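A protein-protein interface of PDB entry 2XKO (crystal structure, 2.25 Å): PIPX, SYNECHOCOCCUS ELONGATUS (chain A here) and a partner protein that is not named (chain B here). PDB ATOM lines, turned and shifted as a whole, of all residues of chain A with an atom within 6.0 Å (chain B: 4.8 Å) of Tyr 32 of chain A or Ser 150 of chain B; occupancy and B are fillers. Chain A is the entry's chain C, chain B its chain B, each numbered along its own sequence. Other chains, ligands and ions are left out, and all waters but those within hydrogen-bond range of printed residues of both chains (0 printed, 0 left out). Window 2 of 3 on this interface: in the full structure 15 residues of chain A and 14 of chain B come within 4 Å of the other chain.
OG of Ser 218 of chain B sits at hydrogen-bond distance from O of Leu 31 of chain A (3.5 Å). The side-chain hydroxyl of Ser 218 of chain B sits at hydrogen-bond distance from the backbone NH of Ala 33 of chain A, 3.2 Å away. The side-chain hydroxyl (OH) of Tyr 32 of chain A is in hydrogen-bond range of the side-chain hydroxyl (OG) of Ser 150 of chain B (3.1 Å).
The backbone carbonyl oxygen (O) of Met 134 of chain B is in hydrogen-bond range of the side-chain hydroxyl (OG1) of Thr 138 of chain B, 3.0 Å away. The side-chain hydroxyl (OG1) of Thr 138 of chain B sits at hydrogen-bond distance from the side-chain hydroxyl (OG) of Ser 150 of chain B, 2.5 Å away. O of Leu 31 of chain A is in hydrogen-bond range of NE2 of Gln 34 of chain A (3.2 Å). The side-chain hydroxyl (OG1) of Thr 30 of chain A is in hydrogen-bond range of the backbone NH (N) of Arg 35 of chain A (3.2 Å).
Met 134 of chain B touches Tyr 32 of chain A. Tyr 32 of chain A touches Leu 153 of chain B. Met 134 of chain B touches Arg 35 of chain A (CG to NH1, 3.8 Å).
Of the printed residues of chain B, Tyr 32 of chain A touches Met 134, Ser 150 and Leu 153. Of the printed residues of chain A, Ser 150 of chain B touches Tyr 32. Of the printed residues of chain A, Leu 153 of chain B touches Tyr 32 (3.9 Å). Of the printed residues of chain A, Ser 218 of chain B touches Leu 31 (3.5 Å) and Ala 33 (3.2 Å). Printed residues of chain A within 4 Å of Met 134 of chain B: Tyr 32 and Arg 35. Val 149 of chain B touches none of the printed residues of chain A. Ser 146 of chain B touches none of the printed residues of chain A.
Hydrophobic or aromatic side chains of chain A that line the printed part of chain B: Tyr 32. Along chain A the printed residues that touch a printed residue of chain B span positions 31 to 35. Among the printed residues, 6 pairs touch across the chains. Among the printed residues, no Asp or Glu carboxylate lies within 4 Å of a Lys or Arg side-chain nitrogen of the other chain.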
ATOM      1  N   LEU A  14       3.665 -30.527  15.015  1.00  0.00           N
ATOM      2  CA  LEU A  14       4.509 -31.522  15.684  1.00  0.00           C
ATOM      3  C   LEU A  14       3.680 -32.642  16.312  1.00  0.00           C
ATOM      4  O   LEU A  14       2.696 -32.407  17.018  1.00  0.00           O
ATOM      5  CB  LEU A  14       5.374 -30.837  16.746  1.00  0.00           C
ATOM      6  CG  LEU A  14       6.727 -31.454  17.070  1.00  0.00           C
ATOM      7  CD1 LEU A  14       7.610 -31.559  15.835  1.00  0.00           C
ATOM      8  CD2 LEU A  14       7.381 -30.610  18.134  1.00  0.00           C
ATOM      9  N   THR A  30      -1.044 -35.782  18.582  1.00  0.00           N
ATOM     10  CA  THR A  30      -0.789 -34.348  18.590  1.00  0.00           C
ATOM     11  C   THR A  30      -0.255 -33.920  19.941  1.00  0.00           C
ATOM     12  O   THR A  30      -0.670 -34.403  20.985  1.00  0.00           O
ATOM     13  CB  THR A  30      -2.033 -33.511  18.243  1.00  0.00           C
ATOM     14  OG1 THR A  30      -3.141 -33.972  19.011  1.00  0.00           O
ATOM     15  CG2 THR A  30      -2.358 -33.640  16.812  1.00  0.00           C
ATOM     16  N   LEU A  31       0.665 -32.979  19.886  1.00  0.00           N
ATOM     17  CA  LEU A  31       1.362 -32.504  21.068  1.00  0.00           C
ATOM     18  C   LEU A  31       0.384 -31.875  22.046  1.00  0.00           C
ATOM     19  O   LEU A  31       0.474 -32.117  23.242  1.00  0.00           O
ATOM     20  CB  LEU A  31       2.418 -31.483  20.655  1.00  0.00           C
ATOM     21  CG  LEU A  31       3.623 -31.346  21.561  1.00  0.00           C
ATOM     22  CD1 LEU A  31       4.447 -32.636  21.528  1.00  0.00           C
ATOM     23  CD2 LEU A  31       4.451 -30.172  21.100  1.00  0.00           C
ATOM     24  N   TYR A  32      -0.568 -31.107  21.522  1.00  0.00           N
ATOM     25  CA  TYR A  32      -1.468 -30.339  22.351  1.00  0.00           C
ATOM     26  C   TYR A  32      -2.639 -31.213  22.793  1.00  0.00           C
ATOM     27  O   TYR A  32      -3.673 -31.259  22.141  1.00  0.00           O
ATOM     28  CB  TYR A  32      -1.949 -29.092  21.589  1.00  0.00           C
ATOM     29  CG  TYR A  32      -2.587 -28.011  22.462  1.00  0.00           C
ATOM     30  CD1 TYR A  32      -1.875 -26.858  22.809  1.00  0.00           C
ATOM     31  CD2 TYR A  32      -3.910 -28.128  22.914  1.00  0.00           C
ATOM     32  CE1 TYR A  32      -2.447 -25.866  23.594  1.00  0.00           C
ATOM     33  CE2 TYR A  32      -4.480 -27.152  23.718  1.00  0.00           C
ATOM     34  CZ  TYR A  32      -3.743 -26.018  24.051  1.00  0.00           C
ATOM     35  OH  TYR A  32      -4.305 -25.038  24.829  1.00  0.00           O
ATOM     36  N   ALA A  33      -2.453 -31.951  23.882  1.00  0.00           N
ATOM     37  CA  ALA A  33      -3.559 -32.664  24.535  1.00  0.00           C
ATOM     38  C   ALA A  33      -4.101 -33.877  23.764  1.00  0.00           C
ATOM     39  O   ALA A  33      -5.177 -34.373  24.075  1.00  0.00           O
ATOM     40  CB  ALA A  33      -4.695 -31.697  24.832  1.00  0.00           C
ATOM     41  N   GLN A  34      -3.374 -34.337  22.760  1.00  0.00           N
ATOM     42  CA  GLN A  34      -3.708 -35.572  22.050  1.00  0.00           C
ATOM     43  C   GLN A  34      -5.154 -35.620  21.513  1.00  0.00           C
ATOM     44  O   GLN A  34      -5.804 -36.669  21.520  1.00  0.00           O
ATOM     45  CB  GLN A  34      -3.422 -36.784  22.928  1.00  0.00           C
ATOM     46  CG  GLN A  34      -1.963 -36.936  23.264  1.00  0.00           C
ATOM     47  CD  GLN A  34      -1.505 -35.982  24.313  1.00  0.00           C
ATOM     48  OE1 GLN A  34      -1.877 -36.118  25.462  1.00  0.00           O
ATOM     49  NE2 GLN A  34      -0.680 -35.001  23.933  1.00  0.00           N
ATOM     50  N   ARG A  35      -5.622 -34.481  21.025  1.00  0.00           N
ATOM     51  CA  ARG A  35      -6.909 -34.380  20.368  1.00  0.00           C
ATOM     52  C   ARG A  35      -6.990 -35.232  19.090  1.00  0.00           C
ATOM     53  O   ARG A  35      -8.077 -35.616  18.664  1.00  0.00           O
ATOM     54  CB  ARG A  35      -7.202 -32.918  20.055  1.00  0.00           C
ATOM     55  CG  ARG A  35      -7.302 -32.036  21.292  1.00  0.00           C
ATOM     56  CD  ARG A  35      -7.594 -30.567  20.947  1.00  0.00           C
ATOM     57  NE  ARG A  35      -7.833 -29.814  22.173  1.00  0.00           N
ATOM     58  CZ  ARG A  35      -8.172 -28.535  22.235  1.00  0.00           C
ATOM     59  NH1 ARG A  35      -8.292 -27.808  21.147  1.00  0.00           N
ATOM     60  NH2 ARG A  35      -8.371 -27.969  23.409  1.00  0.00           N
ATOM     61  N   MET B 134      -7.966 -22.302  18.609  1.00  0.00           N
ATOM     62  CA  MET B 134      -7.037 -22.609  19.694  1.00  0.00           C
ATOM     63  C   MET B 134      -6.411 -21.384  20.306  1.00  0.00           C
ATOM     64  O   MET B 134      -6.152 -21.384  21.488  1.00  0.00           O
ATOM     65  CB  MET B 134      -5.942 -23.605  19.273  1.00  0.00           C
ATOM     66  CG  MET B 134      -6.473 -24.995  19.358  1.00  0.00           C
ATOM     67  SD  MET B 134      -5.371 -26.264  18.729  1.00  0.00           S
ATOM     68  CE  MET B 134      -4.196 -26.337  20.082  1.00  0.00           C
ATOM     69  N   THR B 138      -6.640 -20.102  24.194  1.00  0.00           N
ATOM     70  CA  THR B 138      -5.478 -19.535  24.844  1.00  0.00           C
ATOM     71  C   THR B 138      -5.796 -18.214  25.519  1.00  0.00           C
ATOM     72  O   THR B 138      -5.545 -18.018  26.730  1.00  0.00           O
ATOM     73  CB  THR B 138      -4.350 -19.365  23.805  1.00  0.00           C
ATOM     74  OG1 THR B 138      -3.906 -20.675  23.413  1.00  0.00           O
ATOM     75  CG2 THR B 138      -3.152 -18.528  24.349  1.00  0.00           C
ATOM     76  N   HIS B 141      -8.207 -17.915  28.731  1.00  0.00           N
ATOM     77  CA  HIS B 141      -7.701 -18.154  30.082  1.00  0.00           C
ATOM     78  C   HIS B 141      -7.538 -16.859  30.874  1.00  0.00           C
ATOM     79  O   HIS B 141      -6.898 -15.913  30.418  1.00  0.00           O
ATOM     80  CB  HIS B 141      -6.347 -18.869  30.057  1.00  0.00           C
ATOM     81  CG  HIS B 141      -6.452 -20.331  29.767  1.00  0.00           C
ATOM     82  ND1 HIS B 141      -6.301 -20.858  28.496  1.00  0.00           N
ATOM     83  CD2 HIS B 141      -6.698 -21.379  30.586  1.00  0.00           C
ATOM     84  CE1 HIS B 141      -6.449 -22.170  28.552  1.00  0.00           C
ATOM     85  NE2 HIS B 141      -6.693 -22.509  29.807  1.00  0.00           N
ATOM     86  N   SER B 146      -1.219 -19.403  32.630  1.00  0.00           N
ATOM     87  CA  SER B 146      -1.903 -20.445  31.864  1.00  0.00           C
ATOM     88  C   SER B 146      -1.960 -20.053  30.414  1.00  0.00           C
ATOM     89  O   SER B 146      -1.787 -20.864  29.511  1.00  0.00           O
ATOM     90  CB  SER B 146      -3.339 -20.648  32.375  1.00  0.00           C
ATOM     91  OG  SER B 146      -3.289 -20.975  33.733  1.00  0.00           O
ATOM     92  N   ARG B 147      -2.244 -18.787  30.212  1.00  0.00           N
ATOM     93  CA  ARG B 147      -2.336 -18.257  28.884  1.00  0.00           C
ATOM     94  C   ARG B 147      -0.952 -18.286  28.202  1.00  0.00           C
ATOM     95  O   ARG B 147      -0.850 -18.604  27.027  1.00  0.00           O
ATOM     96  CB  ARG B 147      -2.890 -16.865  28.987  1.00  0.00           C
ATOM     97  CG  ARG B 147      -2.979 -16.172  27.720  1.00  0.00           C
ATOM     98  CD  ARG B 147      -3.451 -14.742  27.916  1.00  0.00           C
ATOM     99  NE  ARG B 147      -4.646 -14.569  28.746  1.00  0.00           N
ATOM    100  CZ  ARG B 147      -5.299 -13.409  28.854  1.00  0.00           C
ATOM    101  NH1 ARG B 147      -4.926 -12.348  28.125  1.00  0.00           N
ATOM    102  NH2 ARG B 147      -6.359 -13.308  29.667  1.00  0.00           N
ATOM    103  N   LEU B 148       0.111 -17.949  28.926  1.00  0.00           N
ATOM    104  CA  LEU B 148       1.460 -18.040  28.338  1.00  0.00           C
ATOM    105  C   LEU B 148       1.795 -19.505  28.011  1.00  0.00           C
ATOM    106  O   LEU B 148       2.203 -19.822  26.892  1.00  0.00           O
ATOM    107  CB  LEU B 148       2.514 -17.390  29.258  1.00  0.00           C
ATOM    108  CG  LEU B 148       3.976 -17.426  28.801  1.00  0.00           C
ATOM    109  CD1 LEU B 148       4.182 -16.714  27.477  1.00  0.00           C
ATOM    110  CD2 LEU B 148       4.891 -16.822  29.892  1.00  0.00           C
ATOM    111  N   VAL B 149       1.581 -20.409  28.959  1.00  0.00           N
ATOM    112  CA  VAL B 149       1.930 -21.800  28.711  1.00  0.00           C
ATOM    113  C   VAL B 149       1.184 -22.314  27.485  1.00  0.00           C
ATOM    114  O   VAL B 149       1.795 -22.896  26.578  1.00  0.00           O
ATOM    115  CB  VAL B 149       1.705 -22.692  29.936  1.00  0.00           C
ATOM    116  CG1 VAL B 149       1.815 -24.175  29.569  1.00  0.00           C
ATOM    117  CG2 VAL B 149       2.725 -22.364  31.015  1.00  0.00           C
ATOM    118  N   SER B 150      -0.121 -22.041  27.419  1.00  0.00           N
ATOM    119  CA  SER B 150      -0.912 -22.476  26.298  1.00  0.00           C
ATOM    120  C   SER B 150      -0.367 -21.947  24.986  1.00  0.00           C
ATOM    121  O   SER B 150      -0.293 -22.672  24.001  1.00  0.00           O
ATOM    122  CB  SER B 150      -2.393 -22.079  26.481  1.00  0.00           C
ATOM    123  OG  SER B 150      -3.080 -22.176  25.251  1.00  0.00           O
ATOM    124  N   PHE B 151      -0.005 -20.678  24.944  1.00  0.00           N
ATOM    125  CA  PHE B 151       0.626 -20.123  23.768  1.00  0.00           C
ATOM    126  C   PHE B 151       1.969 -20.807  23.381  1.00  0.00           C
ATOM    127  O   PHE B 151       2.209 -21.100  22.201  1.00  0.00           O
ATOM    128  CB  PHE B 151       0.884 -18.654  23.979  1.00  0.00           C
ATOM    129  CG  PHE B 151       1.463 -17.976  22.796  1.00  0.00           C
ATOM    130  CD1 PHE B 151       0.795 -17.995  21.556  1.00  0.00           C
ATOM    131  CD2 PHE B 151       2.664 -17.296  22.895  1.00  0.00           C
ATOM    132  CE1 PHE B 151       1.342 -17.333  20.430  1.00  0.00           C
ATOM    133  CE2 PHE B 151       3.200 -16.621  21.778  1.00  0.00           C
ATOM    134  CZ  PHE B 151       2.546 -16.643  20.558  1.00  0.00           C
ATOM    135  N   LEU B 152       2.828 -21.043  24.375  1.00  0.00           N
ATOM    136  CA  LEU B 152       4.101 -21.702  24.139  1.00  0.00           C
ATOM    137  C   LEU B 152       3.879 -23.130  23.660  1.00  0.00           C
ATOM    138  O   LEU B 152       4.599 -23.604  22.816  1.00  0.00           O
ATOM    139  CB  LEU B 152       4.984 -21.701  25.413  1.00  0.00           C
ATOM    140  CG  LEU B 152       5.461 -20.327  25.906  1.00  0.00           C
ATOM    141  CD1 LEU B 152       6.331 -20.513  27.170  1.00  0.00           C
ATOM    142  CD2 LEU B 152       6.218 -19.547  24.829  1.00  0.00           C
ATOM    143  N   LEU B 153       2.866 -23.808  24.196  1.00  0.00           N
ATOM    144  CA  LEU B 153       2.496 -25.150  23.679  1.00  0.00           C
ATOM    145  C   LEU B 153       2.067 -25.101  22.204  1.00  0.00           C
ATOM    146  O   LEU B 153       2.405 -25.991  21.424  1.00  0.00           O
ATOM    147  CB  LEU B 153       1.389 -25.748  24.540  1.00  0.00           C
ATOM    148  CG  LEU B 153       1.814 -26.063  25.989  1.00  0.00           C
ATOM    149  CD1 LEU B 153       0.644 -26.706  26.675  1.00  0.00           C
ATOM    150  CD2 LEU B 153       3.111 -26.962  26.027  1.00  0.00           C
ATOM    151  N   ILE B 154       1.352 -24.041  21.812  1.00  0.00           N
ATOM    152  CA  ILE B 154       1.026 -23.816  20.404  1.00  0.00           C
ATOM    153  C   ILE B 154       2.281 -23.507  19.601  1.00  0.00           C
ATOM    154  O   ILE B 154       2.422 -24.011  18.502  1.00  0.00           O
ATOM    155  CB  ILE B 154      -0.050 -22.741  20.204  1.00  0.00           C
ATOM    156  CG1 ILE B 154      -1.404 -23.241  20.748  1.00  0.00           C
ATOM    157  CG2 ILE B 154      -0.178 -22.381  18.737  1.00  0.00           C
ATOM    158  CD1 ILE B 154      -2.450 -22.151  20.943  1.00  0.00           C
ATOM    159  N   SER B 218       0.765 -30.117  28.722  1.00  0.00           N
ATOM    160  CA  SER B 218      -0.533 -29.979  28.084  1.00  0.00           C
ATOM    161  C   SER B 218      -1.592 -30.754  28.876  1.00  0.00           C
ATOM    162  O   SER B 218      -2.722 -30.311  28.946  1.00  0.00           O
ATOM    163  CB  SER B 218      -0.495 -30.432  26.625  1.00  0.00           C
ATOM    164  OG  SER B 218      -0.602 -31.838  26.542  1.00  0.00           O
ATOM    165  N   PHE B 221      -4.061 -29.033  31.195  1.00  0.00           N
ATOM    166  CA  PHE B 221      -5.028 -28.090  30.605  1.00  0.00           C
ATOM    167  C   PHE B 221      -6.378 -28.707  30.212  1.00  0.00           C
ATOM    168  O   PHE B 221      -7.152 -28.063  29.510  1.00  0.00           O
ATOM    169  CB  PHE B 221      -4.418 -27.458  29.344  1.00  0.00           C
ATOM    170  CG  PHE B 221      -3.396 -26.380  29.632  1.00  0.00           C
ATOM    171  CD1 PHE B 221      -3.711 -25.038  29.445  1.00  0.00           C
ATOM    172  CD2 PHE B 221      -2.133 -26.707  30.099  1.00  0.00           C
ATOM    173  CE1 PHE B 221      -2.798 -24.051  29.713  1.00  0.00           C
ATOM    174  CE2 PHE B 221      -1.196 -25.716  30.370  1.00  0.00           C
ATOM    175  CZ  PHE B 221      -1.534 -24.381  30.171  1.00  0.00           C
